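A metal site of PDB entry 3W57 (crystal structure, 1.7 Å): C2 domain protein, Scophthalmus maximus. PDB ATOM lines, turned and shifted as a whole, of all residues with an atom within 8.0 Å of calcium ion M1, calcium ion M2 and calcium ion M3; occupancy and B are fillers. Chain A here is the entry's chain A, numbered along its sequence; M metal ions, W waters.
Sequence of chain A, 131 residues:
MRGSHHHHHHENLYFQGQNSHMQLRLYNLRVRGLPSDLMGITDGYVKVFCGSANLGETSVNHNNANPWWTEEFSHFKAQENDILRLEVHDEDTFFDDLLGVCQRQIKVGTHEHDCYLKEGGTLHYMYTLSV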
ATOM      1  N   SER A  36       1.516  12.909   1.638  1.00  0.00           N
ATOM      2  CA  SER A  36       0.972  11.656   2.140  1.00  0.00           C
ATOM      3  C   SER A  36      -0.158  11.917   3.140  1.00  0.00           C
ATOM      4  O   SER A  36      -0.159  12.914   3.854  1.00  0.00           O
ATOM      5  CB  SER A  36       2.088  10.865   2.846  1.00  0.00           C
ATOM      6  OG  SER A  36       1.654   9.586   3.303  1.00  0.00           O
ATOM      7  N   ASP A  37      -1.123  11.010   3.172  1.00  0.00           N
ATOM      8  CA  ASP A  37      -2.129  10.936   4.224  1.00  0.00           C
ATOM      9  C   ASP A  37      -1.464  10.232   5.425  1.00  0.00           C
ATOM     10  O   ASP A  37      -0.325   9.773   5.346  1.00  0.00           O
ATOM     11  CB  ASP A  37      -3.313  10.098   3.700  1.00  0.00           C
ATOM     12  CG  ASP A  37      -4.613  10.384   4.414  1.00  0.00           C
ATOM     13  OD1 ASP A  37      -4.597  11.108   5.419  1.00  0.00           O
ATOM     14  OD2 ASP A  37      -5.645   9.851   3.960  1.00  0.00           O
ATOM     15  N   LEU A  38      -2.179  10.168   6.537  1.00  0.00           N
ATOM     16  CA  LEU A  38      -1.718   9.391   7.687  1.00  0.00           C
ATOM     17  C   LEU A  38      -1.497   7.936   7.268  1.00  0.00           C
ATOM     18  O   LEU A  38      -0.545   7.283   7.685  1.00  0.00           O
ATOM     19  CB  LEU A  38      -2.765   9.476   8.792  1.00  0.00           C
ATOM     20  CG  LEU A  38      -2.618   8.571  10.024  1.00  0.00           C
ATOM     21  CD1 LEU A  38      -1.220   8.643  10.615  1.00  0.00           C
ATOM     22  CD2 LEU A  38      -3.671   8.969  11.058  1.00  0.00           C
ATOM     23  N   MET A  39      -2.394   7.431   6.429  1.00  0.00           N
ATOM     24  CA  MET A  39      -2.242   6.094   5.881  1.00  0.00           C
ATOM     25  C   MET A  39      -2.437   6.108   4.381  1.00  0.00           C
ATOM     26  O   MET A  39      -3.565   5.995   3.900  1.00  0.00           O
ATOM     27  CB  MET A  39      -3.263   5.154   6.515  1.00  0.00           C
ATOM     28  CG  MET A  39      -3.052   4.991   7.993  1.00  0.00           C
ATOM     29  SD  MET A  39      -4.253   3.859   8.685  1.00  0.00           S
ATOM     30  CE  MET A  39      -5.749   4.832   8.550  1.00  0.00           C
ATOM     31  N   GLY A  40      -1.338   6.252   3.658  1.00  0.00           N
ATOM     32  CA  GLY A  40      -1.367   6.077   2.225  1.00  0.00           C
ATOM     33  C   GLY A  40      -1.653   7.355   1.466  1.00  0.00           C
ATOM     34  O   GLY A  40      -1.378   8.448   1.942  1.00  0.00           O
ATOM     35  N   ILE A  41      -2.240   7.206   0.281  1.00  0.00           N
ATOM     36  CA  ILE A  41      -2.371   8.326  -0.639  1.00  0.00           C
ATOM     37  C   ILE A  41      -3.608   9.153  -0.327  1.00  0.00           C
ATOM     38  O   ILE A  41      -4.662   8.609  -0.033  1.00  0.00           O
ATOM     39  CB  ILE A  41      -2.385   7.827  -2.095  1.00  0.00           C
ATOM     40  CG1 ILE A  41      -1.133   6.974  -2.337  1.00  0.00           C
ATOM     41  CG2 ILE A  41      -2.476   8.980  -3.083  1.00  0.00           C
ATOM     42  CD1 ILE A  41      -1.082   6.307  -3.699  1.00  0.00           C
ATOM     43  N   THR A  42      -3.456  10.462  -0.367  1.00  0.00           N
ATOM     44  CA  THR A  42      -4.514  11.409  -0.027  1.00  0.00           C
ATOM     45  C   THR A  42      -5.770  11.301  -0.916  1.00  0.00           C
ATOM     46  O   THR A  42      -5.705  10.893  -2.089  1.00  0.00           O
ATOM     47  CB  THR A  42      -3.942  12.834  -0.042  1.00  0.00           C
ATOM     48  OG1 THR A  42      -3.006  12.958   1.025  1.00  0.00           O
ATOM     49  CG2 THR A  42      -5.004  13.894   0.120  1.00  0.00           C
ATOM     50  N   ASP A  43      -6.908  11.672  -0.331  1.00  0.00           N
ATOM     51  CA  ASP A  43      -8.227  11.529  -0.946  1.00  0.00           C
ATOM     52  C   ASP A  43      -8.863  12.907  -1.044  1.00  0.00           C
ATOM     53  O   ASP A  43      -9.742  13.281  -0.253  1.00  0.00           O
ATOM     54  CB  ASP A  43      -9.041  10.595  -0.062  1.00  0.00           C
ATOM     55  CG  ASP A  43      -8.237   9.378   0.330  1.00  0.00           C
ATOM     56  OD1 ASP A  43      -7.986   8.560  -0.576  1.00  0.00           O
ATOM     57  OD2 ASP A  43      -7.805   9.265   1.500  1.00  0.00           O
ATOM     58  N   GLY A  44      -8.398  13.686  -2.013  1.00  0.00           N
ATOM     59  CA  GLY A  44      -8.724  15.099  -2.070  1.00  0.00           C
ATOM     60  C   GLY A  44     -10.090  15.458  -2.610  1.00  0.00           C
ATOM     61  O   GLY A  44     -10.636  14.772  -3.481  1.00  0.00           O
ATOM     62  N   VAL A  60     -14.834  13.227  -4.161  1.00  0.00           N
ATOM     63  CA  VAL A  60     -13.528  12.857  -3.634  1.00  0.00           C
ATOM     64  C   VAL A  60     -12.787  12.076  -4.711  1.00  0.00           C
ATOM     65  O   VAL A  60     -13.357  11.166  -5.356  1.00  0.00           O
ATOM     66  CB  VAL A  60     -13.686  11.989  -2.358  1.00  0.00           C
ATOM     67  CG1 VAL A  60     -12.339  11.507  -1.863  1.00  0.00           C
ATOM     68  CG2 VAL A  60     -14.404  12.764  -1.257  1.00  0.00           C
ATOM     69  N   ASN A  61     -11.534  12.459  -4.942  1.00  0.00           N
ATOM     70  CA  ASN A  61     -10.694  11.770  -5.907  1.00  0.00           C
ATOM     71  C   ASN A  61      -9.789  10.848  -5.105  1.00  0.00           C
ATOM     72  O   ASN A  61      -8.725  11.239  -4.634  1.00  0.00           O
ATOM     73  CB  ASN A  61      -9.899  12.800  -6.735  1.00  0.00           C
ATOM     74  CG  ASN A  61      -9.379  12.216  -8.029  1.00  0.00           C
ATOM     75  OD1 ASN A  61      -8.920  11.097  -8.055  1.00  0.00           O
ATOM     76  ND2 ASN A  61      -9.456  12.999  -9.109  1.00  0.00           N
ATOM     77  N   HIS A  62     -10.252   9.617  -4.888  1.00  0.00           N
ATOM     78  CA  HIS A  62      -9.622   8.715  -3.934  1.00  0.00           C
ATOM     79  C   HIS A  62      -8.225   8.271  -4.328  1.00  0.00           C
ATOM     80  O   HIS A  62      -7.968   8.006  -5.507  1.00  0.00           O
ATOM     81  CB  HIS A  62     -10.485   7.473  -3.726  1.00  0.00           C
ATOM     82  CG  HIS A  62     -11.796   7.768  -3.064  1.00  0.00           C
ATOM     83  ND1 HIS A  62     -11.912   7.885  -1.693  1.00  0.00           N
ATOM     84  CD2 HIS A  62     -13.028   8.025  -3.573  1.00  0.00           C
ATOM     85  CE1 HIS A  62     -13.175   8.167  -1.388  1.00  0.00           C
ATOM     86  NE2 HIS A  62     -13.857   8.253  -2.507  1.00  0.00           N
ATOM     87  N   ASN A  63      -7.351   8.249  -3.330  1.00  0.00           N
ATOM     88  CA  ASN A  63      -6.006   7.688  -3.492  1.00  0.00           C
ATOM     89  C   ASN A  63      -5.290   8.252  -4.710  1.00  0.00           C
ATOM     90  O   ASN A  63      -4.795   7.496  -5.555  1.00  0.00           O
ATOM     91  CB  ASN A  63      -6.103   6.182  -3.580  1.00  0.00           C
ATOM     92  CG  ASN A  63      -6.694   5.595  -2.345  1.00  0.00           C
ATOM     93  OD1 ASN A  63      -6.286   5.949  -1.249  1.00  0.00           O
ATOM     94  ND2 ASN A  63      -7.701   4.719  -2.498  1.00  0.00           N
ATOM     95  N   ASN A  64      -5.242   9.573  -4.765  1.00  0.00           N
ATOM     96  CA  ASN A  64      -4.658  10.267  -5.895  1.00  0.00           C
ATOM     97  C   ASN A  64      -3.834  11.465  -5.412  1.00  0.00           C
ATOM     98  O   ASN A  64      -4.383  12.412  -4.865  1.00  0.00           O
ATOM     99  CB  ASN A  64      -5.782  10.715  -6.844  1.00  0.00           C
ATOM    100  CG  ASN A  64      -5.280  11.128  -8.232  1.00  0.00           C
ATOM    101  OD1 ASN A  64      -4.101  11.435  -8.409  1.00  0.00           O
ATOM    102  ND2 ASN A  64      -6.197  11.167  -9.209  1.00  0.00           N
ATOM    103  N   HIS A  89      -9.400  19.724   0.805  1.00  0.00           N
ATOM    104  CA  HIS A  89      -9.491  18.859   1.976  1.00  0.00           C
ATOM    105  C   HIS A  89      -9.127  17.437   1.601  1.00  0.00           C
ATOM    106  O   HIS A  89      -9.294  17.028   0.459  1.00  0.00           O
ATOM    107  CB  HIS A  89     -10.922  18.805   2.526  1.00  0.00           C
ATOM    108  CG  HIS A  89     -11.453  20.120   3.021  1.00  0.00           C
ATOM    109  ND1 HIS A  89     -11.651  20.379   4.363  1.00  0.00           N
ATOM    110  CD2 HIS A  89     -11.871  21.223   2.359  1.00  0.00           C
ATOM    111  CE1 HIS A  89     -12.154  21.589   4.504  1.00  0.00           C
ATOM    112  NE2 HIS A  89     -12.299  22.133   3.308  1.00  0.00           N
ATOM    113  N   ASP A  90      -8.656  16.687   2.602  1.00  0.00           N
ATOM    114  CA  ASP A  90      -8.540  15.228   2.497  1.00  0.00           C
ATOM    115  C   ASP A  90      -9.737  14.592   3.201  1.00  0.00           C
ATOM    116  O   ASP A  90      -9.963  14.866   4.381  1.00  0.00           O
ATOM    117  CB  ASP A  90      -7.271  14.751   3.170  1.00  0.00           C
ATOM    118  CG  ASP A  90      -7.233  13.247   3.345  1.00  0.00           C
ATOM    119  OD1 ASP A  90      -7.392  12.521   2.344  1.00  0.00           O
ATOM    120  OD2 ASP A  90      -7.112  12.766   4.492  1.00  0.00           O
ATOM    121  N   GLU A  91     -10.481  13.730   2.499  1.00  0.00           N
ATOM    122  CA  GLU A  91     -11.543  12.982   3.156  1.00  0.00           C
ATOM    123  C   GLU A  91     -10.969  11.880   4.034  1.00  0.00           C
ATOM    124  O   GLU A  91     -10.114  11.115   3.590  1.00  0.00           O
ATOM    125  CB  GLU A  91     -12.503  12.364   2.125  1.00  0.00           C
ATOM    126  CG  GLU A  91     -13.720  11.726   2.774  1.00  0.00           C
ATOM    127  CD  GLU A  91     -14.528  10.861   1.819  1.00  0.00           C
ATOM    128  OE1 GLU A  91     -15.713  11.181   1.597  1.00  0.00           O
ATOM    129  OE2 GLU A  91     -13.981   9.860   1.307  1.00  0.00           O
ATOM    130  N   ASP A  92     -11.437  11.823   5.280  1.00  0.00           N
ATOM    131  CA  ASP A  92     -11.088  10.742   6.197  1.00  0.00           C
ATOM    132  C   ASP A  92     -12.336  10.231   6.902  1.00  0.00           C
ATOM    133  O   ASP A  92     -13.402  10.851   6.848  1.00  0.00           O
ATOM    134  CB  ASP A  92     -10.121  11.241   7.250  1.00  0.00           C
ATOM    135  CG  ASP A  92      -8.666  11.174   6.809  1.00  0.00           C
ATOM    136  OD1 ASP A  92      -8.277  10.244   6.073  1.00  0.00           O
ATOM    137  OD2 ASP A  92      -7.935  12.052   7.264  1.00  0.00           O
ATOM    138  N   THR A  93     -12.204   9.078   7.548  1.00  0.00           N
ATOM    139  CA  THR A  93     -13.358   8.439   8.204  1.00  0.00           C
ATOM    140  C   THR A  93     -13.972   9.268   9.337  1.00  0.00           C
ATOM    141  O   THR A  93     -15.209   9.375   9.427  1.00  0.00           O
ATOM    142  CB  THR A  93     -12.992   7.041   8.692  1.00  0.00           C
ATOM    143  OG1 THR A  93     -12.659   6.226   7.552  1.00  0.00           O
ATOM    144  CG2 THR A  93     -14.174   6.408   9.412  1.00  0.00           C
ATOM    145  N   PHE A  95     -12.525  12.612  10.805  1.00  0.00           N
ATOM    146  CA  PHE A  95     -12.400  14.067  10.637  1.00  0.00           C
ATOM    147  C   PHE A  95     -11.651  14.346   9.349  1.00  0.00           C
ATOM    148  O   PHE A  95     -10.539  13.878   9.183  1.00  0.00           O
ATOM    149  CB  PHE A  95     -11.609  14.719  11.774  1.00  0.00           C
ATOM    150  CG  PHE A  95     -12.179  14.450  13.151  1.00  0.00           C
ATOM    151  CD1 PHE A  95     -13.119  15.297  13.705  1.00  0.00           C
ATOM    152  CD2 PHE A  95     -11.754  13.350  13.871  1.00  0.00           C
ATOM    153  CE1 PHE A  95     -13.634  15.043  14.979  1.00  0.00           C
ATOM    154  CE2 PHE A  95     -12.256  13.085  15.143  1.00  0.00           C
ATOM    155  CZ  PHE A  95     -13.183  13.930  15.692  1.00  0.00           C
ATOM    156  N   ASP A  96     -12.242  15.134   8.442  1.00  0.00           N
ATOM    157  CA  ASP A  96     -11.509  15.525   7.231  1.00  0.00           C
ATOM    158  C   ASP A  96     -10.437  16.547   7.590  1.00  0.00           C
ATOM    159  O   ASP A  96     -10.630  17.356   8.513  1.00  0.00           O
ATOM    160  CB  ASP A  96     -12.457  16.126   6.188  1.00  0.00           C
ATOM    161  CG  ASP A  96     -13.420  15.128   5.602  1.00  0.00           C
ATOM    162  OD1 ASP A  96     -13.327  13.921   5.918  1.00  0.00           O
ATOM    163  OD2 ASP A  96     -14.291  15.534   4.801  1.00  0.00           O
ATOM    164  N   ASP A  97      -9.313  16.527   6.875  1.00  0.00           N
ATOM    165  CA  ASP A  97      -8.205  17.444   7.142  1.00  0.00           C
ATOM    166  C   ASP A  97      -8.147  18.529   6.069  1.00  0.00           C
ATOM    167  O   ASP A  97      -8.112  18.222   4.879  1.00  0.00           O
ATOM    168  CB  ASP A  97      -6.875  16.702   7.132  1.00  0.00           C
ATOM    169  CG  ASP A  97      -6.732  15.773   8.301  1.00  0.00           C
ATOM    170  OD1 ASP A  97      -6.898  16.241   9.447  1.00  0.00           O
ATOM    171  OD2 ASP A  97      -6.498  14.567   8.072  1.00  0.00           O
ATOM    172  N   LEU A  98      -8.093  19.779   6.507  1.00  0.00           N
ATOM    173  CA  LEU A  98      -7.970  20.879   5.561  1.00  0.00           C
ATOM    174  C   LEU A  98      -6.500  21.073   5.229  1.00  0.00           C
ATOM    175  O   LEU A  98      -5.679  21.337   6.118  1.00  0.00           O
ATOM    176  CB  LEU A  98      -8.618  22.149   6.149  1.00  0.00           C
ATOM    177  CG  LEU A  98      -8.554  23.449   5.340  1.00  0.00           C
ATOM    178  CD1 LEU A  98      -8.913  23.251   3.865  1.00  0.00           C
ATOM    179  CD2 LEU A  98      -9.467  24.464   5.964  1.00  0.00           C
ATOM    180  N   LEU A  99      -6.155  20.901   3.941  1.00  0.00           N
ATOM    181  CA  LEU A  99      -4.766  20.934   3.513  1.00  0.00           C
ATOM    182  C   LEU A  99      -4.298  22.307   3.070  1.00  0.00           C
ATOM    183  O   LEU A  99      -3.113  22.617   3.177  1.00  0.00           O
ATOM    184  CB  LEU A  99      -4.530  19.932   2.388  1.00  0.00           C
ATOM    185  CG  LEU A  99      -5.013  18.501   2.625  1.00  0.00           C
ATOM    186  CD1 LEU A  99      -4.664  17.641   1.425  1.00  0.00           C
ATOM    187  CD2 LEU A  99      -4.411  17.906   3.882  1.00  0.00           C
HETATM  188 CA    CA M   1      -5.790  12.823   6.651  1.00  0.00          CA
HETATM  189 CA    CA M   2      -7.872  10.416   3.666  1.00  0.00          CA
HETATM  190 CA    CA M   3      -6.424   7.208   0.745  1.00  0.00          CA
HETATM  191  O   HOH W   1      -8.690   8.005   4.024  1.00  0.00           O
HETATM  192  O   HOH W   2      -5.454   7.403   2.970  1.00  0.00           O
HETATM  193  O   HOH W   3      -3.455  13.051   7.558  1.00  0.00           O
HETATM  194  O   HOH W   4      -8.464   6.168   1.643  1.00  0.00           O
HETATM  195  O   HOH W   5      -5.434   5.005   1.270  1.00  0.00           O
HETATM  196  O   HOH W   6      -5.520  11.492   8.870  1.00  0.00           O
HETATM  197  O   HOH W   7      -4.695  14.717   5.446  1.00  0.00           O
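N of Asp 37 sits at hydrogen-bond distance from OG1 of Thr 42. The backbone NH (N) of Asp 92 lies within hydrogen-bond range of the side-chain carboxylate (OD1) of Asp 96, 2.9 Å away. The backbone NH of Asn 63 lies within hydrogen-bond range of the backbone carbonyl oxygen of Thr 42, at 3.4 Å.
Of the 24 residues printed, 4 come within 4 Å of calcium ion M1.
Calcium ion M3 is bound by the side-chain amide oxygen (OD1) of Asn 63 (2.4 Å), the backbone carbonyl oxygen (O) of Ile 41 (2.4 Å), water W2 (2.4 Å), the side-chain carboxylate (OD1) of Asp 43 (2.5 Å), water W4 (2.5 Å), water W5 (2.5 Å) and the side-chain carboxylate (OD2) of Asp 43 (2.6 Å). Calcium ion M3 has seven donor atoms within binding distance.
Calcium ion M1 is bound by OD2 of Asp 97 (2.4 Å), OD2 of Asp 92 (2.4 Å), OD1 of Asp 37 (2.4 Å), water W7 (2.5 Å), water W3 (2.5 Å), OD2 of Asp 90 (2.5 Å) and water W6 (2.6 Å).
Three residues have an atom within 4 Å of calcium ion M3: Ile 41, Asp 43 and Asn 63.
Of the 24 residues printed, 5 come within 4 Å of calcium ion M2. The nearest printed residue that does not touch calcium ion M2 is Thr 42 (5.1 Å).
OD2 of Asp 37 is bound to calcium ion M2. Calcium ion M2 is bound by the backbone carbonyl oxygen (O) of Glu 91, at 2.3 Å. Calcium ion M2 is bound by OD1 of Asp 92. Calcium ion M2 is bound by OD2 of Asp 43 (2.5 Å). OD1 of Asp 90 binds calcium ion M2, 2.5 Å away. Water W1 binds calcium ion M2 (2.6 Å). OD2 of Asp 90 binds calcium ion M2 (2.6 Å). Calcium ion M2 has seven donor atoms within binding distance.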
